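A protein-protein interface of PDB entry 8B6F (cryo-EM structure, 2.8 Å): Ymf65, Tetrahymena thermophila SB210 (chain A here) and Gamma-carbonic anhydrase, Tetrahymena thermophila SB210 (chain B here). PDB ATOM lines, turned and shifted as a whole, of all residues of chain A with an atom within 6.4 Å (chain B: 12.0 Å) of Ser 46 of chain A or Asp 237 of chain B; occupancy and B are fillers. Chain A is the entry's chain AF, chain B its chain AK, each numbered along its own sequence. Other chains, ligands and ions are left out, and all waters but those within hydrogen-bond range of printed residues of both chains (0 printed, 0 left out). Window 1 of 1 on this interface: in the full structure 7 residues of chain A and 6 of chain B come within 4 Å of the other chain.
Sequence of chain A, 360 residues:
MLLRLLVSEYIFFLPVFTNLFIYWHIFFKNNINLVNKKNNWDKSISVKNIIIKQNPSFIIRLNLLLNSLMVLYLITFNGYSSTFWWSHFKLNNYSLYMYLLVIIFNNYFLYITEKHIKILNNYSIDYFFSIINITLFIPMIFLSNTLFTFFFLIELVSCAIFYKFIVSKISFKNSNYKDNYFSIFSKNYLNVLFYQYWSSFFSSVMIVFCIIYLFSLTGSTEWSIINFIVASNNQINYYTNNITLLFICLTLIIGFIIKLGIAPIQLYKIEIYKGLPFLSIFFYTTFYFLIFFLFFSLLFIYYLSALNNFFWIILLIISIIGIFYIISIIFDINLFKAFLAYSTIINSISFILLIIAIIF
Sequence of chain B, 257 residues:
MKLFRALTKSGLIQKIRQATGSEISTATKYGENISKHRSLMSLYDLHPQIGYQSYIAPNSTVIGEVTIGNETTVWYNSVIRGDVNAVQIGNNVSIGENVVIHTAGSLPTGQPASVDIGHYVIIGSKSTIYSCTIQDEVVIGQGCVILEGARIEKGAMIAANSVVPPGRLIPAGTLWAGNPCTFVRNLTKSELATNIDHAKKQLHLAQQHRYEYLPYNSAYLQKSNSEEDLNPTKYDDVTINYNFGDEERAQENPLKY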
ATOM      1  N   LYS A  38     -28.137  12.216   1.314  1.00  0.00           N
ATOM      2  CA  LYS A  38     -29.199  11.577   0.544  1.00  0.00           C
ATOM      3  C   LYS A  38     -30.324  12.590   0.367  1.00  0.00           C
ATOM      4  O   LYS A  38     -31.052  12.891   1.319  1.00  0.00           O
ATOM      5  CB  LYS A  38     -29.700  10.315   1.245  1.00  0.00           C
ATOM      6  CG  LYS A  38     -30.873   9.640   0.548  1.00  0.00           C
ATOM      7  CD  LYS A  38     -31.329   8.405   1.307  1.00  0.00           C
ATOM      8  CE  LYS A  38     -32.574   7.803   0.680  1.00  0.00           C
ATOM      9  NZ  LYS A  38     -33.041   6.593   1.411  1.00  0.00           N
ATOM     10  N   SER A  44     -32.661   4.686  -2.130  1.00  0.00           N
ATOM     11  CA  SER A  44     -31.581   3.804  -1.702  1.00  0.00           C
ATOM     12  C   SER A  44     -31.929   2.367  -2.065  1.00  0.00           C
ATOM     13  O   SER A  44     -32.968   1.850  -1.642  1.00  0.00           O
ATOM     14  CB  SER A  44     -31.333   3.925  -0.199  1.00  0.00           C
ATOM     15  OG  SER A  44     -30.874   5.221   0.140  1.00  0.00           O
ATOM     16  N   ILE A  45     -31.057   1.725  -2.843  1.00  0.00           N
ATOM     17  CA  ILE A  45     -31.272   0.328  -3.201  1.00  0.00           C
ATOM     18  C   ILE A  45     -31.157  -0.560  -1.969  1.00  0.00           C
ATOM     19  O   ILE A  45     -31.867  -1.564  -1.841  1.00  0.00           O
ATOM     20  CB  ILE A  45     -30.287  -0.094  -4.308  1.00  0.00           C
ATOM     21  CG1 ILE A  45     -30.640  -1.492  -4.820  1.00  0.00           C
ATOM     22  CG2 ILE A  45     -28.850  -0.043  -3.798  1.00  0.00           C
ATOM     23  CD1 ILE A  45     -29.826  -1.935  -6.020  1.00  0.00           C
ATOM     24  N   SER A  46     -30.261  -0.210  -1.050  1.00  0.00           N
ATOM     25  CA  SER A  46     -30.064  -0.960   0.181  1.00  0.00           C
ATOM     26  C   SER A  46     -29.924   0.019   1.337  1.00  0.00           C
ATOM     27  O   SER A  46     -29.641   1.203   1.143  1.00  0.00           O
ATOM     28  CB  SER A  46     -28.834  -1.874   0.094  1.00  0.00           C
ATOM     29  OG  SER A  46     -27.675  -1.142  -0.259  1.00  0.00           O
ATOM     30  N   VAL A  47     -30.139  -0.487   2.549  1.00  0.00           N
ATOM     31  CA  VAL A  47     -30.008   0.342   3.742  1.00  0.00           C
ATOM     32  C   VAL A  47     -28.534   0.624   3.997  1.00  0.00           C
ATOM     33  O   VAL A  47     -27.702  -0.292   4.009  1.00  0.00           O
ATOM     34  CB  VAL A  47     -30.666  -0.343   4.949  1.00  0.00           C
ATOM     35  CG1 VAL A  47     -30.442   0.466   6.219  1.00  0.00           C
ATOM     36  CG2 VAL A  47     -32.152  -0.540   4.702  1.00  0.00           C
ATOM     37  N   LYS A  48     -28.205   1.896   4.208  1.00  0.00           N
ATOM     38  CA  LYS A  48     -26.817   2.286   4.412  1.00  0.00           C
ATOM     39  C   LYS A  48     -26.254   1.643   5.672  1.00  0.00           C
ATOM     40  O   LYS A  48     -26.923   1.564   6.705  1.00  0.00           O
ATOM     41  CB  LYS A  48     -26.706   3.808   4.509  1.00  0.00           C
ATOM     42  CG  LYS A  48     -25.302   4.308   4.821  1.00  0.00           C
ATOM     43  CD  LYS A  48     -25.245   5.825   4.842  1.00  0.00           C
ATOM     44  CE  LYS A  48     -23.844   6.318   5.157  1.00  0.00           C
ATOM     45  NZ  LYS A  48     -23.778   7.805   5.191  1.00  0.00           N
ATOM     46  N   ASN A  49     -25.007   1.188   5.579  1.00  0.00           N
ATOM     47  CA  ASN A  49     -24.278   0.625   6.713  1.00  0.00           C
ATOM     48  C   ASN A  49     -23.395   1.728   7.283  1.00  0.00           C
ATOM     49  O   ASN A  49     -22.309   2.001   6.768  1.00  0.00           O
ATOM     50  CB  ASN A  49     -23.461  -0.587   6.280  1.00  0.00           C
ATOM     51  CG  ASN A  49     -22.651  -1.178   7.412  1.00  0.00           C
ATOM     52  OD1 ASN A  49     -23.183  -1.874   8.274  1.00  0.00           O
ATOM     53  ND2 ASN A  49     -21.351  -0.915   7.406  1.00  0.00           N
ATOM     54  N   ILE A  50     -23.872   2.369   8.352  1.00  0.00           N
ATOM     55  CA  ILE A  50     -23.153   3.499   8.931  1.00  0.00           C
ATOM     56  C   ILE A  50     -21.851   3.047   9.583  1.00  0.00           C
ATOM     57  O   ILE A  50     -20.867   3.795   9.599  1.00  0.00           O
ATOM     58  CB  ILE A  50     -24.057   4.252   9.926  1.00  0.00           C
ATOM     59  CG1 ILE A  50     -24.543   3.313  11.037  1.00  0.00           C
ATOM     60  CG2 ILE A  50     -25.231   4.876   9.182  1.00  0.00           C
ATOM     61  CD1 ILE A  50     -25.449   3.973  12.058  1.00  0.00           C
ATOM     62  N   ILE A  52     -18.481   1.422   9.616  1.00  0.00           N
ATOM     63  CA  ILE A  52     -17.511   1.106   8.574  1.00  0.00           C
ATOM     64  C   ILE A  52     -16.126   0.997   9.195  1.00  0.00           C
ATOM     65  O   ILE A  52     -15.783   1.749  10.114  1.00  0.00           O
ATOM     66  CB  ILE A  52     -17.521   2.159   7.446  1.00  0.00           C
ATOM     67  CG1 ILE A  52     -17.202   3.550   8.003  1.00  0.00           C
ATOM     68  CG2 ILE A  52     -18.873   2.163   6.747  1.00  0.00           C
ATOM     69  CD1 ILE A  52     -16.976   4.597   6.934  1.00  0.00           C
ATOM     70  N   PRO B 232     -33.139 -10.554  -6.639  1.00  0.00           N
ATOM     71  CA  PRO B 232     -33.240 -10.581  -5.176  1.00  0.00           C
ATOM     72  C   PRO B 232     -34.442  -9.792  -4.678  1.00  0.00           C
ATOM     73  O   PRO B 232     -34.839  -8.783  -5.264  1.00  0.00           O
ATOM     74  CB  PRO B 232     -31.925  -9.942  -4.712  1.00  0.00           C
ATOM     75  CG  PRO B 232     -31.007 -10.044  -5.874  1.00  0.00           C
ATOM     76  CD  PRO B 232     -31.872  -9.951  -7.086  1.00  0.00           C
ATOM     77  N   THR B 233     -35.025 -10.270  -3.576  1.00  0.00           N
ATOM     78  CA  THR B 233     -36.141  -9.556  -2.967  1.00  0.00           C
ATOM     79  C   THR B 233     -35.670  -8.283  -2.274  1.00  0.00           C
ATOM     80  O   THR B 233     -36.293  -7.224  -2.417  1.00  0.00           O
ATOM     81  CB  THR B 233     -36.864 -10.465  -1.973  1.00  0.00           C
ATOM     82  OG1 THR B 233     -37.304 -11.656  -2.640  1.00  0.00           O
ATOM     83  CG2 THR B 233     -38.068  -9.756  -1.366  1.00  0.00           C
ATOM     84  N   LYS B 234     -34.574  -8.367  -1.523  1.00  0.00           N
ATOM     85  CA  LYS B 234     -34.016  -7.231  -0.807  1.00  0.00           C
ATOM     86  C   LYS B 234     -32.515  -7.175  -1.046  1.00  0.00           C
ATOM     87  O   LYS B 234     -31.874  -8.197  -1.301  1.00  0.00           O
ATOM     88  CB  LYS B 234     -34.302  -7.318   0.696  1.00  0.00           C
ATOM     89  CG  LYS B 234     -33.815  -8.606   1.342  1.00  0.00           C
ATOM     90  CD  LYS B 234     -34.247  -8.702   2.800  1.00  0.00           C
ATOM     91  CE  LYS B 234     -33.520  -7.699   3.684  1.00  0.00           C
ATOM     92  NZ  LYS B 234     -32.050  -7.939   3.726  1.00  0.00           N
ATOM     93  N   TYR B 235     -31.961  -5.971  -0.957  1.00  0.00           N
ATOM     94  CA  TYR B 235     -30.548  -5.733  -1.199  1.00  0.00           C
ATOM     95  C   TYR B 235     -29.862  -5.271   0.078  1.00  0.00           C
ATOM     96  O   TYR B 235     -30.466  -4.606   0.925  1.00  0.00           O
ATOM     97  CB  TYR B 235     -30.348  -4.689  -2.301  1.00  0.00           C
ATOM     98  CG  TYR B 235     -30.771  -5.165  -3.670  1.00  0.00           C
ATOM     99  CD1 TYR B 235     -32.102  -5.124  -4.060  1.00  0.00           C
ATOM    100  CD2 TYR B 235     -29.837  -5.653  -4.573  1.00  0.00           C
ATOM    101  CE1 TYR B 235     -32.492  -5.560  -5.312  1.00  0.00           C
ATOM    102  CE2 TYR B 235     -30.216  -6.091  -5.825  1.00  0.00           C
ATOM    103  CZ  TYR B 235     -31.544  -6.040  -6.190  1.00  0.00           C
ATOM    104  OH  TYR B 235     -31.924  -6.477  -7.437  1.00  0.00           O
ATOM    105  N   ASP B 236     -28.590  -5.634   0.207  1.00  0.00           N
ATOM    106  CA  ASP B 236     -27.766  -5.271   1.348  1.00  0.00           C
ATOM    107  C   ASP B 236     -26.668  -4.312   0.912  1.00  0.00           C
ATOM    108  O   ASP B 236     -26.363  -4.177  -0.275  1.00  0.00           O
ATOM    109  CB  ASP B 236     -27.141  -6.510   1.995  1.00  0.00           C
ATOM    110  CG  ASP B 236     -28.179  -7.471   2.540  1.00  0.00           C
ATOM    111  OD1 ASP B 236     -29.225  -7.002   3.035  1.00  0.00           O
ATOM    112  OD2 ASP B 236     -27.947  -8.695   2.480  1.00  0.00           O
ATOM    113  N   ASP B 237     -26.077  -3.638   1.894  1.00  0.00           N
ATOM    114  CA  ASP B 237     -24.976  -2.720   1.645  1.00  0.00           C
ATOM    115  C   ASP B 237     -23.658  -3.482   1.636  1.00  0.00           C
ATOM    116  O   ASP B 237     -23.417  -4.341   2.489  1.00  0.00           O
ATOM    117  CB  ASP B 237     -24.941  -1.618   2.706  1.00  0.00           C
ATOM    118  CG  ASP B 237     -23.952  -0.521   2.371  1.00  0.00           C
ATOM    119  OD1 ASP B 237     -24.146   0.163   1.345  1.00  0.00           O
ATOM    120  OD2 ASP B 237     -22.980  -0.337   3.132  1.00  0.00           O
ATOM    121  N   VAL B 238     -22.810  -3.170   0.660  1.00  0.00           N
ATOM    122  CA  VAL B 238     -21.531  -3.860   0.515  1.00  0.00           C
ATOM    123  C   VAL B 238     -20.630  -3.455   1.679  1.00  0.00           C
ATOM    124  O   VAL B 238     -20.194  -2.305   1.775  1.00  0.00           O
ATOM    125  CB  VAL B 238     -20.878  -3.564  -0.842  1.00  0.00           C
ATOM    126  CG1 VAL B 238     -21.761  -4.061  -1.971  1.00  0.00           C
ATOM    127  CG2 VAL B 238     -20.594  -2.075  -1.026  1.00  0.00           C
ATOM    128  N   THR B 239     -20.378  -4.396   2.590  1.00  0.00           N
ATOM    129  CA  THR B 239     -19.485  -4.171   3.721  1.00  0.00           C
ATOM    130  C   THR B 239     -18.113  -4.794   3.488  1.00  0.00           C
ATOM    131  O   THR B 239     -17.105  -4.086   3.439  1.00  0.00           O
ATOM    132  CB  THR B 239     -20.110  -4.734   5.005  1.00  0.00           C
ATOM    133  OG1 THR B 239     -20.309  -6.147   4.870  1.00  0.00           O
ATOM    134  CG2 THR B 239     -21.442  -4.060   5.292  1.00  0.00           C
ATOM    135  N   ILE B 240     -18.060  -6.113   3.335  1.00  0.00           N
ATOM    136  CA  ILE B 240     -16.804  -6.813   3.102  1.00  0.00           C
ATOM    137  C   ILE B 240     -17.134  -8.198   2.567  1.00  0.00           C
ATOM    138  O   ILE B 240     -18.113  -8.821   2.982  1.00  0.00           O
ATOM    139  CB  ILE B 240     -15.952  -6.882   4.393  1.00  0.00           C
ATOM    140  CG1 ILE B 240     -14.594  -7.538   4.125  1.00  0.00           C
ATOM    141  CG2 ILE B 240     -16.685  -7.653   5.480  1.00  0.00           C
ATOM    142  CD1 ILE B 240     -13.690  -6.732   3.231  1.00  0.00           C
ATOM    143  N   ASN B 241     -16.306  -8.675   1.644  1.00  0.00           N
ATOM    144  CA  ASN B 241     -16.444 -10.021   1.108  1.00  0.00           C
ATOM    145  C   ASN B 241     -15.665 -10.982   1.990  1.00  0.00           C
ATOM    146  O   ASN B 241     -14.490 -10.747   2.288  1.00  0.00           O
ATOM    147  CB  ASN B 241     -15.934 -10.091  -0.330  1.00  0.00           C
ATOM    148  CG  ASN B 241     -16.829  -9.357  -1.302  1.00  0.00           C
ATOM    149  OD1 ASN B 241     -17.692  -8.578  -0.903  1.00  0.00           O
ATOM    150  ND2 ASN B 241     -16.623  -9.597  -2.590  1.00  0.00           N
ATOM    151  N   TYR B 242     -16.322 -12.064   2.409  1.00  0.00           N
ATOM    152  CA  TYR B 242     -15.661 -13.012   3.296  1.00  0.00           C
ATOM    153  C   TYR B 242     -14.377 -13.547   2.682  1.00  0.00           C
ATOM    154  O   TYR B 242     -13.435 -13.881   3.408  1.00  0.00           O
ATOM    155  CB  TYR B 242     -16.606 -14.163   3.642  1.00  0.00           C
ATOM    156  CG  TYR B 242     -16.806 -15.150   2.518  1.00  0.00           C
ATOM    157  CD1 TYR B 242     -17.672 -14.876   1.471  1.00  0.00           C
ATOM    158  CD2 TYR B 242     -16.128 -16.361   2.511  1.00  0.00           C
ATOM    159  CE1 TYR B 242     -17.853 -15.779   0.443  1.00  0.00           C
ATOM    160  CE2 TYR B 242     -16.302 -17.269   1.489  1.00  0.00           C
ATOM    161  CZ  TYR B 242     -17.167 -16.973   0.459  1.00  0.00           C
ATOM    162  OH  TYR B 242     -17.342 -17.879  -0.559  1.00  0.00           O
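Of the 9 printed residues of chain A, 4 touch a printed residue of chain B. Printed residues of chain A that touch a printed residue of chain B: Ile 45, Ser 46, Val 47 and Asn 49. Of the 11 printed residues of chain B, 4 touch a printed residue of chain A.
Among the printed residues, pairs that only touch across the chains: Ile 45 of chain A with Tyr 235 of chain B, Ser 46 of chain A with Tyr 235 of chain B, Ser 46 of chain A with Asp 237 of chain B, Val 47 of chain A with Asp 237 of chain B, Asn 49 of chain A with Asp 237 of chain B and Asn 49 of chain A with Thr 239 of chain B.
The side-chain hydroxyl (OG) of Ser 46 of chain A lies within hydrogen-bond range of the backbone carbonyl oxygen (O) of Asp 236 of chain B, 3.3 Å away.
The side-chain amino group (NZ) of Lys 234 of chain B lies within salt-bridge range of the side-chain carboxylate (OD1) of Asp 236 of chain B (3.1 Å).
Ser 46 of chain A touches just these residues of chain B: Tyr 235, Asp 236 and Asp 237. Ser 44 of chain A touches none of the printed residues of chain B. Ile 45 of chain A touches just one residue of chain B: Tyr 235. Asn 49 of chain A touches just these residues of chain B: Asp 237 and Thr 239. Printed residues of chain A within 4 Å of Thr 239 of chain B: Asn 49. Of the printed residues of chain A, Asp 236 of chain B touches Ser 46 (3.3 Å). Of the printed residues of chain A, Tyr 235 of chain B touches Ile 45 and Ser 46. Val 238 of chain B touches none of the printed residues of chain A. Ile 50 of chain A touches none of the printed residues of chain B. The nearest residue of chain A that does not touch Asp 237 of chain B is Lys 48 of chain A (4.5 Å).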
